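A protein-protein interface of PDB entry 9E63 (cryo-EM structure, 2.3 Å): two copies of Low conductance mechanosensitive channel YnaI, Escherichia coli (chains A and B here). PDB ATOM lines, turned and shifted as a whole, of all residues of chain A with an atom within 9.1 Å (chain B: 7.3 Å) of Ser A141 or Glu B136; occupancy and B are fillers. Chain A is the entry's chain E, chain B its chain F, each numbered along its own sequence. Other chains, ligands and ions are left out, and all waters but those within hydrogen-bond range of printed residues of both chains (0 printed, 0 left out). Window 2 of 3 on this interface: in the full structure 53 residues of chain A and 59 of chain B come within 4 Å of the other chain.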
ATOM      1  N   LEU A 132     -17.385 -13.674   2.057  1.00  0.00           N
ATOM      2  CA  LEU A 132     -17.412 -13.824   3.507  1.00  0.00           C
ATOM      3  C   LEU A 132     -17.093 -15.258   3.916  1.00  0.00           C
ATOM      4  O   LEU A 132     -16.537 -15.495   4.995  1.00  0.00           O
ATOM      5  CB  LEU A 132     -18.778 -13.383   4.040  1.00  0.00           C
ATOM      6  CG  LEU A 132     -19.124 -13.397   5.534  1.00  0.00           C
ATOM      7  CD1 LEU A 132     -19.721 -14.734   5.950  1.00  0.00           C
ATOM      8  CD2 LEU A 132     -17.925 -13.034   6.403  1.00  0.00           C
ATOM      9  N   GLY A 135     -12.976 -16.184   2.684  1.00  0.00           N
ATOM     10  CA  GLY A 135     -12.082 -15.092   3.012  1.00  0.00           C
ATOM     11  C   GLY A 135     -10.764 -15.497   3.637  1.00  0.00           C
ATOM     12  O   GLY A 135     -10.076 -14.657   4.224  1.00  0.00           O
ATOM     13  N   GLU A 136     -10.394 -16.773   3.531  1.00  0.00           N
ATOM     14  CA  GLU A 136      -9.145 -17.226   4.131  1.00  0.00           C
ATOM     15  C   GLU A 136      -8.290 -18.021   3.152  1.00  0.00           C
ATOM     16  O   GLU A 136      -7.058 -17.981   3.228  1.00  0.00           O
ATOM     17  CB  GLU A 136      -9.435 -18.064   5.375  1.00  0.00           C
ATOM     18  CG  GLU A 136     -10.709 -18.870   5.276  1.00  0.00           C
ATOM     19  CD  GLU A 136     -10.570 -20.079   4.375  1.00  0.00           C
ATOM     20  OE1 GLU A 136      -9.911 -21.059   4.785  1.00  0.00           O
ATOM     21  OE2 GLU A 136     -11.113 -20.047   3.252  1.00  0.00           O
ATOM     22  N   HIS A 137      -8.928 -18.749   2.233  1.00  0.00           N
ATOM     23  CA  HIS A 137      -8.171 -19.541   1.267  1.00  0.00           C
ATOM     24  C   HIS A 137      -7.348 -18.641   0.356  1.00  0.00           C
ATOM     25  O   HIS A 137      -6.208 -18.971   0.005  1.00  0.00           O
ATOM     26  CB  HIS A 137      -9.116 -20.423   0.452  1.00  0.00           C
ATOM     27  CG  HIS A 137      -9.590 -21.638   1.190  1.00  0.00           C
ATOM     28  ND1 HIS A 137     -10.899 -21.801   1.593  1.00  0.00           N
ATOM     29  CD2 HIS A 137      -8.932 -22.748   1.597  1.00  0.00           C
ATOM     30  CE1 HIS A 137     -11.024 -22.957   2.217  1.00  0.00           C
ATOM     31  NE2 HIS A 137      -9.845 -23.553   2.232  1.00  0.00           N
ATOM     32  N   PHE A 138      -7.913 -17.504  -0.043  1.00  0.00           N
ATOM     33  CA  PHE A 138      -7.202 -16.488  -0.807  1.00  0.00           C
ATOM     34  C   PHE A 138      -7.464 -15.092  -0.253  1.00  0.00           C
ATOM     35  O   PHE A 138      -7.150 -14.096  -0.908  1.00  0.00           O
ATOM     36  CB  PHE A 138      -7.600 -16.561  -2.281  1.00  0.00           C
ATOM     37  CG  PHE A 138      -9.058 -16.846  -2.495  1.00  0.00           C
ATOM     38  CD1 PHE A 138     -10.014 -15.874  -2.237  1.00  0.00           C
ATOM     39  CD2 PHE A 138      -9.476 -18.086  -2.943  1.00  0.00           C
ATOM     40  CE1 PHE A 138     -11.355 -16.135  -2.430  1.00  0.00           C
ATOM     41  CE2 PHE A 138     -10.819 -18.352  -3.138  1.00  0.00           C
ATOM     42  CZ  PHE A 138     -11.758 -17.374  -2.881  1.00  0.00           C
ATOM     43  N   GLY A 139      -8.032 -15.005   0.947  1.00  0.00           N
ATOM     44  CA  GLY A 139      -8.527 -13.745   1.456  1.00  0.00           C
ATOM     45  C   GLY A 139      -7.609 -13.040   2.430  1.00  0.00           C
ATOM     46  O   GLY A 139      -6.386 -13.034   2.258  1.00  0.00           O
ATOM     47  N   MET A 140      -8.199 -12.446   3.466  1.00  0.00           N
ATOM     48  CA  MET A 140      -7.471 -11.551   4.355  1.00  0.00           C
ATOM     49  C   MET A 140      -7.513 -12.050   5.792  1.00  0.00           C
ATOM     50  O   MET A 140      -7.944 -13.177   6.053  1.00  0.00           O
ATOM     51  CB  MET A 140      -8.058 -10.143   4.265  1.00  0.00           C
ATOM     52  CG  MET A 140      -7.030  -9.051   4.101  1.00  0.00           C
ATOM     53  SD  MET A 140      -6.673  -8.825   2.350  1.00  0.00           S
ATOM     54  CE  MET A 140      -8.155  -7.969   1.818  1.00  0.00           C
ATOM     55  N   SER A 141      -7.063 -11.219   6.726  1.00  0.00           N
ATOM     56  CA  SER A 141      -7.052 -11.602   8.130  1.00  0.00           C
ATOM     57  C   SER A 141      -8.470 -11.723   8.665  1.00  0.00           C
ATOM     58  O   SER A 141      -9.354 -10.944   8.303  1.00  0.00           O
ATOM     59  CB  SER A 141      -6.274 -10.583   8.957  1.00  0.00           C
ATOM     60  OG  SER A 141      -6.486 -10.780  10.344  1.00  0.00           O
ATOM     61  N   LEU A 142      -8.680 -12.701   9.543  1.00  0.00           N
ATOM     62  CA  LEU A 142     -10.010 -12.932  10.089  1.00  0.00           C
ATOM     63  C   LEU A 142     -10.281 -12.009  11.269  1.00  0.00           C
ATOM     64  O   LEU A 142     -10.737 -12.460  12.325  1.00  0.00           O
ATOM     65  CB  LEU A 142     -10.167 -14.394  10.512  1.00  0.00           C
ATOM     66  CG  LEU A 142     -10.284 -15.456   9.412  1.00  0.00           C
ATOM     67  CD1 LEU A 142     -11.120 -14.949   8.247  1.00  0.00           C
ATOM     68  CD2 LEU A 142      -8.914 -15.920   8.939  1.00  0.00           C
ATOM     69  N   SER A 143     -10.003 -10.729  11.108  1.00  0.00           N
ATOM     70  CA  SER A 143     -10.468  -9.712  12.045  1.00  0.00           C
ATOM     71  C   SER A 143     -11.148  -8.550  11.344  1.00  0.00           C
ATOM     72  O   SER A 143     -12.151  -8.039  11.846  1.00  0.00           O
ATOM     73  CB  SER A 143      -9.303  -9.194  12.899  1.00  0.00           C
ATOM     74  OG  SER A 143      -9.605  -7.926  13.454  1.00  0.00           O
ATOM     75  N   GLY A 144     -10.625  -8.115  10.197  1.00  0.00           N
ATOM     76  CA  GLY A 144     -11.348  -7.150   9.389  1.00  0.00           C
ATOM     77  C   GLY A 144     -12.591  -7.750   8.761  1.00  0.00           C
ATOM     78  O   GLY A 144     -13.640  -7.101   8.692  1.00  0.00           O
ATOM     79  N   LEU A 145     -12.488  -8.995   8.294  1.00  0.00           N
ATOM     80  CA  LEU A 145     -13.648  -9.671   7.723  1.00  0.00           C
ATOM     81  C   LEU A 145     -14.739  -9.859   8.765  1.00  0.00           C
ATOM     82  O   LEU A 145     -15.927  -9.686   8.469  1.00  0.00           O
ATOM     83  CB  LEU A 145     -13.228 -11.013   7.127  1.00  0.00           C
ATOM     84  CG  LEU A 145     -12.388 -10.933   5.851  1.00  0.00           C
ATOM     85  CD1 LEU A 145     -12.459 -12.239   5.086  1.00  0.00           C
ATOM     86  CD2 LEU A 145     -12.833  -9.775   4.970  1.00  0.00           C
ATOM     87  N   LEU A 146     -14.354 -10.208   9.995  1.00  0.00           N
ATOM     88  CA  LEU A 146     -15.331 -10.325  11.074  1.00  0.00           C
ATOM     89  C   LEU A 146     -16.070  -9.013  11.286  1.00  0.00           C
ATOM     90  O   LEU A 146     -17.298  -8.993  11.399  1.00  0.00           O
ATOM     91  CB  LEU A 146     -14.640 -10.758  12.366  1.00  0.00           C
ATOM     92  CG  LEU A 146     -14.617 -12.240  12.739  1.00  0.00           C
ATOM     93  CD1 LEU A 146     -14.448 -12.399  14.244  1.00  0.00           C
ATOM     94  CD2 LEU A 146     -15.877 -12.941  12.267  1.00  0.00           C
ATOM     95  N   THR A 147     -15.335  -7.901  11.335  1.00  0.00           N
ATOM     96  CA  THR A 147     -15.958  -6.603  11.574  1.00  0.00           C
ATOM     97  C   THR A 147     -16.880  -6.209  10.426  1.00  0.00           C
ATOM     98  O   THR A 147     -18.004  -5.735  10.647  1.00  0.00           O
ATOM     99  CB  THR A 147     -14.881  -5.539  11.776  1.00  0.00           C
ATOM    100  OG1 THR A 147     -14.269  -5.715  13.058  1.00  0.00           O
ATOM    101  CG2 THR A 147     -15.484  -4.156  11.682  1.00  0.00           C
ATOM    102  N   PHE A 148     -16.413  -6.385   9.189  1.00  0.00           N
ATOM    103  CA  PHE A 148     -17.225  -6.036   8.028  1.00  0.00           C
ATOM    104  C   PHE A 148     -18.511  -6.848   8.007  1.00  0.00           C
ATOM    105  O   PHE A 148     -19.610  -6.297   7.839  1.00  0.00           O
ATOM    106  CB  PHE A 148     -16.418  -6.266   6.751  1.00  0.00           C
ATOM    107  CG  PHE A 148     -16.849  -5.415   5.593  1.00  0.00           C
ATOM    108  CD1 PHE A 148     -17.382  -4.155   5.801  1.00  0.00           C
ATOM    109  CD2 PHE A 148     -16.721  -5.876   4.294  1.00  0.00           C
ATOM    110  CE1 PHE A 148     -17.776  -3.370   4.736  1.00  0.00           C
ATOM    111  CE2 PHE A 148     -17.115  -5.098   3.225  1.00  0.00           C
ATOM    112  CZ  PHE A 148     -17.644  -3.842   3.446  1.00  0.00           C
ATOM    113  N   THR B  83       3.332  -6.085  -0.229  1.00  0.00           N
ATOM    114  CA  THR B  83       2.000  -5.713   0.240  1.00  0.00           C
ATOM    115  C   THR B  83       1.755  -4.219   0.079  1.00  0.00           C
ATOM    116  O   THR B  83       0.654  -3.798  -0.298  1.00  0.00           O
ATOM    117  CB  THR B  83       1.816  -6.131   1.698  1.00  0.00           C
ATOM    118  OG1 THR B  83       2.939  -5.689   2.469  1.00  0.00           O
ATOM    119  CG2 THR B  83       1.691  -7.644   1.804  1.00  0.00           C
ATOM    120  N   VAL B 131      -8.282   0.193   5.321  1.00  0.00           N
ATOM    121  CA  VAL B 131      -7.463   0.115   6.529  1.00  0.00           C
ATOM    122  C   VAL B 131      -8.014  -0.942   7.475  1.00  0.00           C
ATOM    123  O   VAL B 131      -7.257  -1.671   8.129  1.00  0.00           O
ATOM    124  CB  VAL B 131      -7.370   1.496   7.202  1.00  0.00           C
ATOM    125  CG1 VAL B 131      -6.751   1.379   8.583  1.00  0.00           C
ATOM    126  CG2 VAL B 131      -6.552   2.443   6.341  1.00  0.00           C
ATOM    127  N   LEU B 132      -9.342  -1.049   7.559  1.00  0.00           N
ATOM    128  CA  LEU B 132      -9.944  -2.105   8.365  1.00  0.00           C
ATOM    129  C   LEU B 132      -9.581  -3.484   7.823  1.00  0.00           C
ATOM    130  O   LEU B 132      -9.422  -4.440   8.591  1.00  0.00           O
ATOM    131  CB  LEU B 132     -11.462  -1.907   8.414  1.00  0.00           C
ATOM    132  CG  LEU B 132     -12.396  -2.862   9.168  1.00  0.00           C
ATOM    133  CD1 LEU B 132     -12.860  -4.006   8.277  1.00  0.00           C
ATOM    134  CD2 LEU B 132     -11.763  -3.385  10.453  1.00  0.00           C
ATOM    135  N   LEU B 133      -9.443  -3.607   6.501  1.00  0.00           N
ATOM    136  CA  LEU B 133      -9.078  -4.894   5.914  1.00  0.00           C
ATOM    137  C   LEU B 133      -7.569  -5.131   5.931  1.00  0.00           C
ATOM    138  O   LEU B 133      -7.122  -6.268   6.113  1.00  0.00           O
ATOM    139  CB  LEU B 133      -9.615  -4.991   4.487  1.00  0.00           C
ATOM    140  CG  LEU B 133     -11.110  -5.272   4.329  1.00  0.00           C
ATOM    141  CD1 LEU B 133     -11.388  -5.950   2.999  1.00  0.00           C
ATOM    142  CD2 LEU B 133     -11.624  -6.128   5.475  1.00  0.00           C
ATOM    143  N   TYR B 134      -6.773  -4.081   5.741  1.00  0.00           N
ATOM    144  CA  TYR B 134      -5.314  -4.174   5.689  1.00  0.00           C
ATOM    145  C   TYR B 134      -4.667  -3.768   7.009  1.00  0.00           C
ATOM    146  O   TYR B 134      -3.601  -3.150   7.029  1.00  0.00           O
ATOM    147  CB  TYR B 134      -4.749  -3.319   4.558  1.00  0.00           C
ATOM    148  CG  TYR B 134      -4.923  -3.895   3.174  1.00  0.00           C
ATOM    149  CD1 TYR B 134      -5.434  -5.170   2.986  1.00  0.00           C
ATOM    150  CD2 TYR B 134      -4.561  -3.165   2.051  1.00  0.00           C
ATOM    151  CE1 TYR B 134      -5.585  -5.699   1.722  1.00  0.00           C
ATOM    152  CE2 TYR B 134      -4.711  -3.685   0.780  1.00  0.00           C
ATOM    153  CZ  TYR B 134      -5.224  -4.953   0.622  1.00  0.00           C
ATOM    154  OH  TYR B 134      -5.377  -5.481  -0.638  1.00  0.00           O
ATOM    155  N   GLY B 135      -5.300  -4.109   8.124  1.00  0.00           N
ATOM    156  CA  GLY B 135      -4.812  -3.667   9.413  1.00  0.00           C
ATOM    157  C   GLY B 135      -3.818  -4.592  10.084  1.00  0.00           C
ATOM    158  O   GLY B 135      -3.595  -4.484  11.293  1.00  0.00           O
ATOM    159  N   GLU B 136      -3.219  -5.513   9.328  1.00  0.00           N
ATOM    160  CA  GLU B 136      -2.261  -6.437   9.925  1.00  0.00           C
ATOM    161  C   GLU B 136      -0.957  -6.518   9.140  1.00  0.00           C
ATOM    162  O   GLU B 136       0.108  -6.730   9.728  1.00  0.00           O
ATOM    163  CB  GLU B 136      -2.884  -7.827  10.045  1.00  0.00           C
ATOM    164  CG  GLU B 136      -3.851  -8.153   8.930  1.00  0.00           C
ATOM    165  CD  GLU B 136      -3.153  -8.471   7.623  1.00  0.00           C
ATOM    166  OE1 GLU B 136      -2.566  -9.568   7.511  1.00  0.00           O
ATOM    167  OE2 GLU B 136      -3.187  -7.620   6.712  1.00  0.00           O
ATOM    168  N   HIS B 137      -1.024  -6.356   7.815  1.00  0.00           N
ATOM    169  CA  HIS B 137       0.186  -6.443   7.003  1.00  0.00           C
ATOM    170  C   HIS B 137       1.160  -5.330   7.360  1.00  0.00           C
ATOM    171  O   HIS B 137       2.374  -5.551   7.432  1.00  0.00           O
ATOM    172  CB  HIS B 137      -0.170  -6.394   5.519  1.00  0.00           C
ATOM    173  CG  HIS B 137      -0.706  -7.686   4.982  1.00  0.00           C
ATOM    174  ND1 HIS B 137      -2.022  -7.847   4.606  1.00  0.00           N
ATOM    175  CD2 HIS B 137      -0.103  -8.877   4.760  1.00  0.00           C
ATOM    176  CE1 HIS B 137      -2.207  -9.082   4.176  1.00  0.00           C
ATOM    177  NE2 HIS B 137      -1.058  -9.728   4.258  1.00  0.00           N
ATOM    178  N   PHE B 138       0.640  -4.127   7.586  1.00  0.00           N
ATOM    179  CA  PHE B 138       1.413  -3.002   8.098  1.00  0.00           C
ATOM    180  C   PHE B 138       0.704  -2.339   9.271  1.00  0.00           C
ATOM    181  O   PHE B 138       1.065  -1.228   9.668  1.00  0.00           O
ATOM    182  CB  PHE B 138       1.659  -1.983   6.984  1.00  0.00           C
ATOM    183  CG  PHE B 138       0.489  -1.807   6.062  1.00  0.00           C
ATOM    184  CD1 PHE B 138      -0.639  -1.116   6.476  1.00  0.00           C
ATOM    185  CD2 PHE B 138       0.509  -2.338   4.784  1.00  0.00           C
ATOM    186  CE1 PHE B 138      -1.720  -0.957   5.634  1.00  0.00           C
ATOM    187  CE2 PHE B 138      -0.570  -2.180   3.936  1.00  0.00           C
ATOM    188  CZ  PHE B 138      -1.686  -1.488   4.363  1.00  0.00           C
ATOM    189  N   GLY B 139      -0.298  -3.008   9.833  1.00  0.00           N
ATOM    190  CA  GLY B 139      -1.210  -2.366  10.756  1.00  0.00           C
ATOM    191  C   GLY B 139      -0.926  -2.592  12.223  1.00  0.00           C
ATOM    192  O   GLY B 139       0.222  -2.508  12.670  1.00  0.00           O
ATOM    193  N   MET B 140      -1.978  -2.893  12.981  1.00  0.00           N
ATOM    194  CA  MET B 140      -1.915  -2.833  14.434  1.00  0.00           C
ATOM    195  C   MET B 140      -2.364  -4.151  15.049  1.00  0.00           C
ATOM    196  O   MET B 140      -2.568  -5.138  14.334  1.00  0.00           O
ATOM    197  CB  MET B 140      -2.793  -1.687  14.935  1.00  0.00           C
ATOM    198  CG  MET B 140      -2.297  -0.996  16.184  1.00  0.00           C
ATOM    199  SD  MET B 140      -0.859  -0.002  15.768  1.00  0.00           S
ATOM    200  CE  MET B 140      -1.665   1.537  15.332  1.00  0.00           C
ATOM    201  N   SER B 141      -2.520  -4.179  16.369  1.00  0.00           N
ATOM    202  CA  SER B 141      -3.029  -5.368  17.034  1.00  0.00           C
ATOM    203  C   SER B 141      -4.508  -5.551  16.731  1.00  0.00           C
ATOM    204  O   SER B 141      -5.271  -4.584  16.674  1.00  0.00           O
ATOM    205  CB  SER B 141      -2.822  -5.268  18.541  1.00  0.00           C
ATOM    206  OG  SER B 141      -3.531  -6.284  19.225  1.00  0.00           O
ATOM    207  N   LEU B 142      -4.916  -6.806  16.554  1.00  0.00           N
ATOM    208  CA  LEU B 142      -6.296  -7.091  16.189  1.00  0.00           C
ATOM    209  C   LEU B 142      -7.193  -7.127  17.419  1.00  0.00           C
ATOM    210  O   LEU B 142      -7.983  -8.061  17.591  1.00  0.00           O
ATOM    211  CB  LEU B 142      -6.385  -8.418  15.431  1.00  0.00           C
ATOM    212  CG  LEU B 142      -5.854  -8.466  13.996  1.00  0.00           C
ATOM    213  CD1 LEU B 142      -6.158  -7.175  13.254  1.00  0.00           C
ATOM    214  CD2 LEU B 142      -4.361  -8.767  13.971  1.00  0.00           C
ATOM    215  N   LEU B 145      -8.411  -2.590  16.593  1.00  0.00           N
ATOM    216  CA  LEU B 145      -9.087  -2.521  15.303  1.00  0.00           C
ATOM    217  C   LEU B 145     -10.468  -3.153  15.376  1.00  0.00           C
ATOM    218  O   LEU B 145     -11.430  -2.628  14.805  1.00  0.00           O
ATOM    219  CB  LEU B 145      -8.236  -3.193  14.228  1.00  0.00           C
ATOM    220  CG  LEU B 145      -6.963  -2.441  13.833  1.00  0.00           C
ATOM    221  CD1 LEU B 145      -6.487  -2.888  12.467  1.00  0.00           C
ATOM    222  CD2 LEU B 145      -7.186  -0.935  13.853  1.00  0.00           C
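The backbone carbonyl oxygen (O) of Gly A135 is in hydrogen-bond range of the backbone NH (N) of Met A140.
A ring nitrogen (ND1) of His B137 is in hydrogen-bond range of the side-chain carboxylate of Glu B136, 2.4 Å away.
The backbone carbonyl oxygen (O) of Ser A143 sits at hydrogen-bond distance from the side-chain hydroxyl (OG1) of Thr A147, at 3.4 Å.
Among the printed residues, merely in contact across the chains: Met A140 with Leu B133, Met A140 with Tyr B134, Ser A141 with Glu B136, Ser A143 with Leu B142, Gly A144 with Leu B132, Gly A144 with Leu B133, Leu A145 with Leu B133 and Thr A147 with Leu B132.
Ser A141 touches just one residue of chain B: Glu B136.
Glu B136 touches just one residue of chain A: Ser A141 (3.4 Å).
No residue of chain A comes within 4 Å of His B137.
Of the printed residues of chain B, Met A140 touches Leu B133 and Tyr B134.
Printed residues of chain B within 4 Å of Gly A144: Leu B132 and Leu B133.
Of the printed residues of chain A, Tyr B134 touches Met A140 (3.4 Å).
Of the printed residues of chain A, Leu B133 touches Met A140 (3.4 Å), Gly A144 (3.8 Å) and Leu A145 (3.9 Å).
Printed residues of chain A within 4 Å of Leu B132: Gly A144 and Thr A147.
Thr B83 touches none of the printed residues of chain A.
Glu A136 touches none of the printed residues of chain B.
The nearest printed residue of chain B that does not touch Ser A143 is Leu B132 (4.9 Å).
Hydrophobic or aromatic side chains of chain A that line the printed part of chain B: Met A140 and Leu A145.
Ser A141 touches Glu B136, but with the chains exchanged Glu A136 does not touch Ser B141 (17.6 Å).
Positions printed for both chains: 132, 135, 136, 137, 138, 139, 140, 141, 142 and 145.
Of the 8 pairs that touch across the chains among the printed residues, none has its exchanged pair printed and touching as well.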
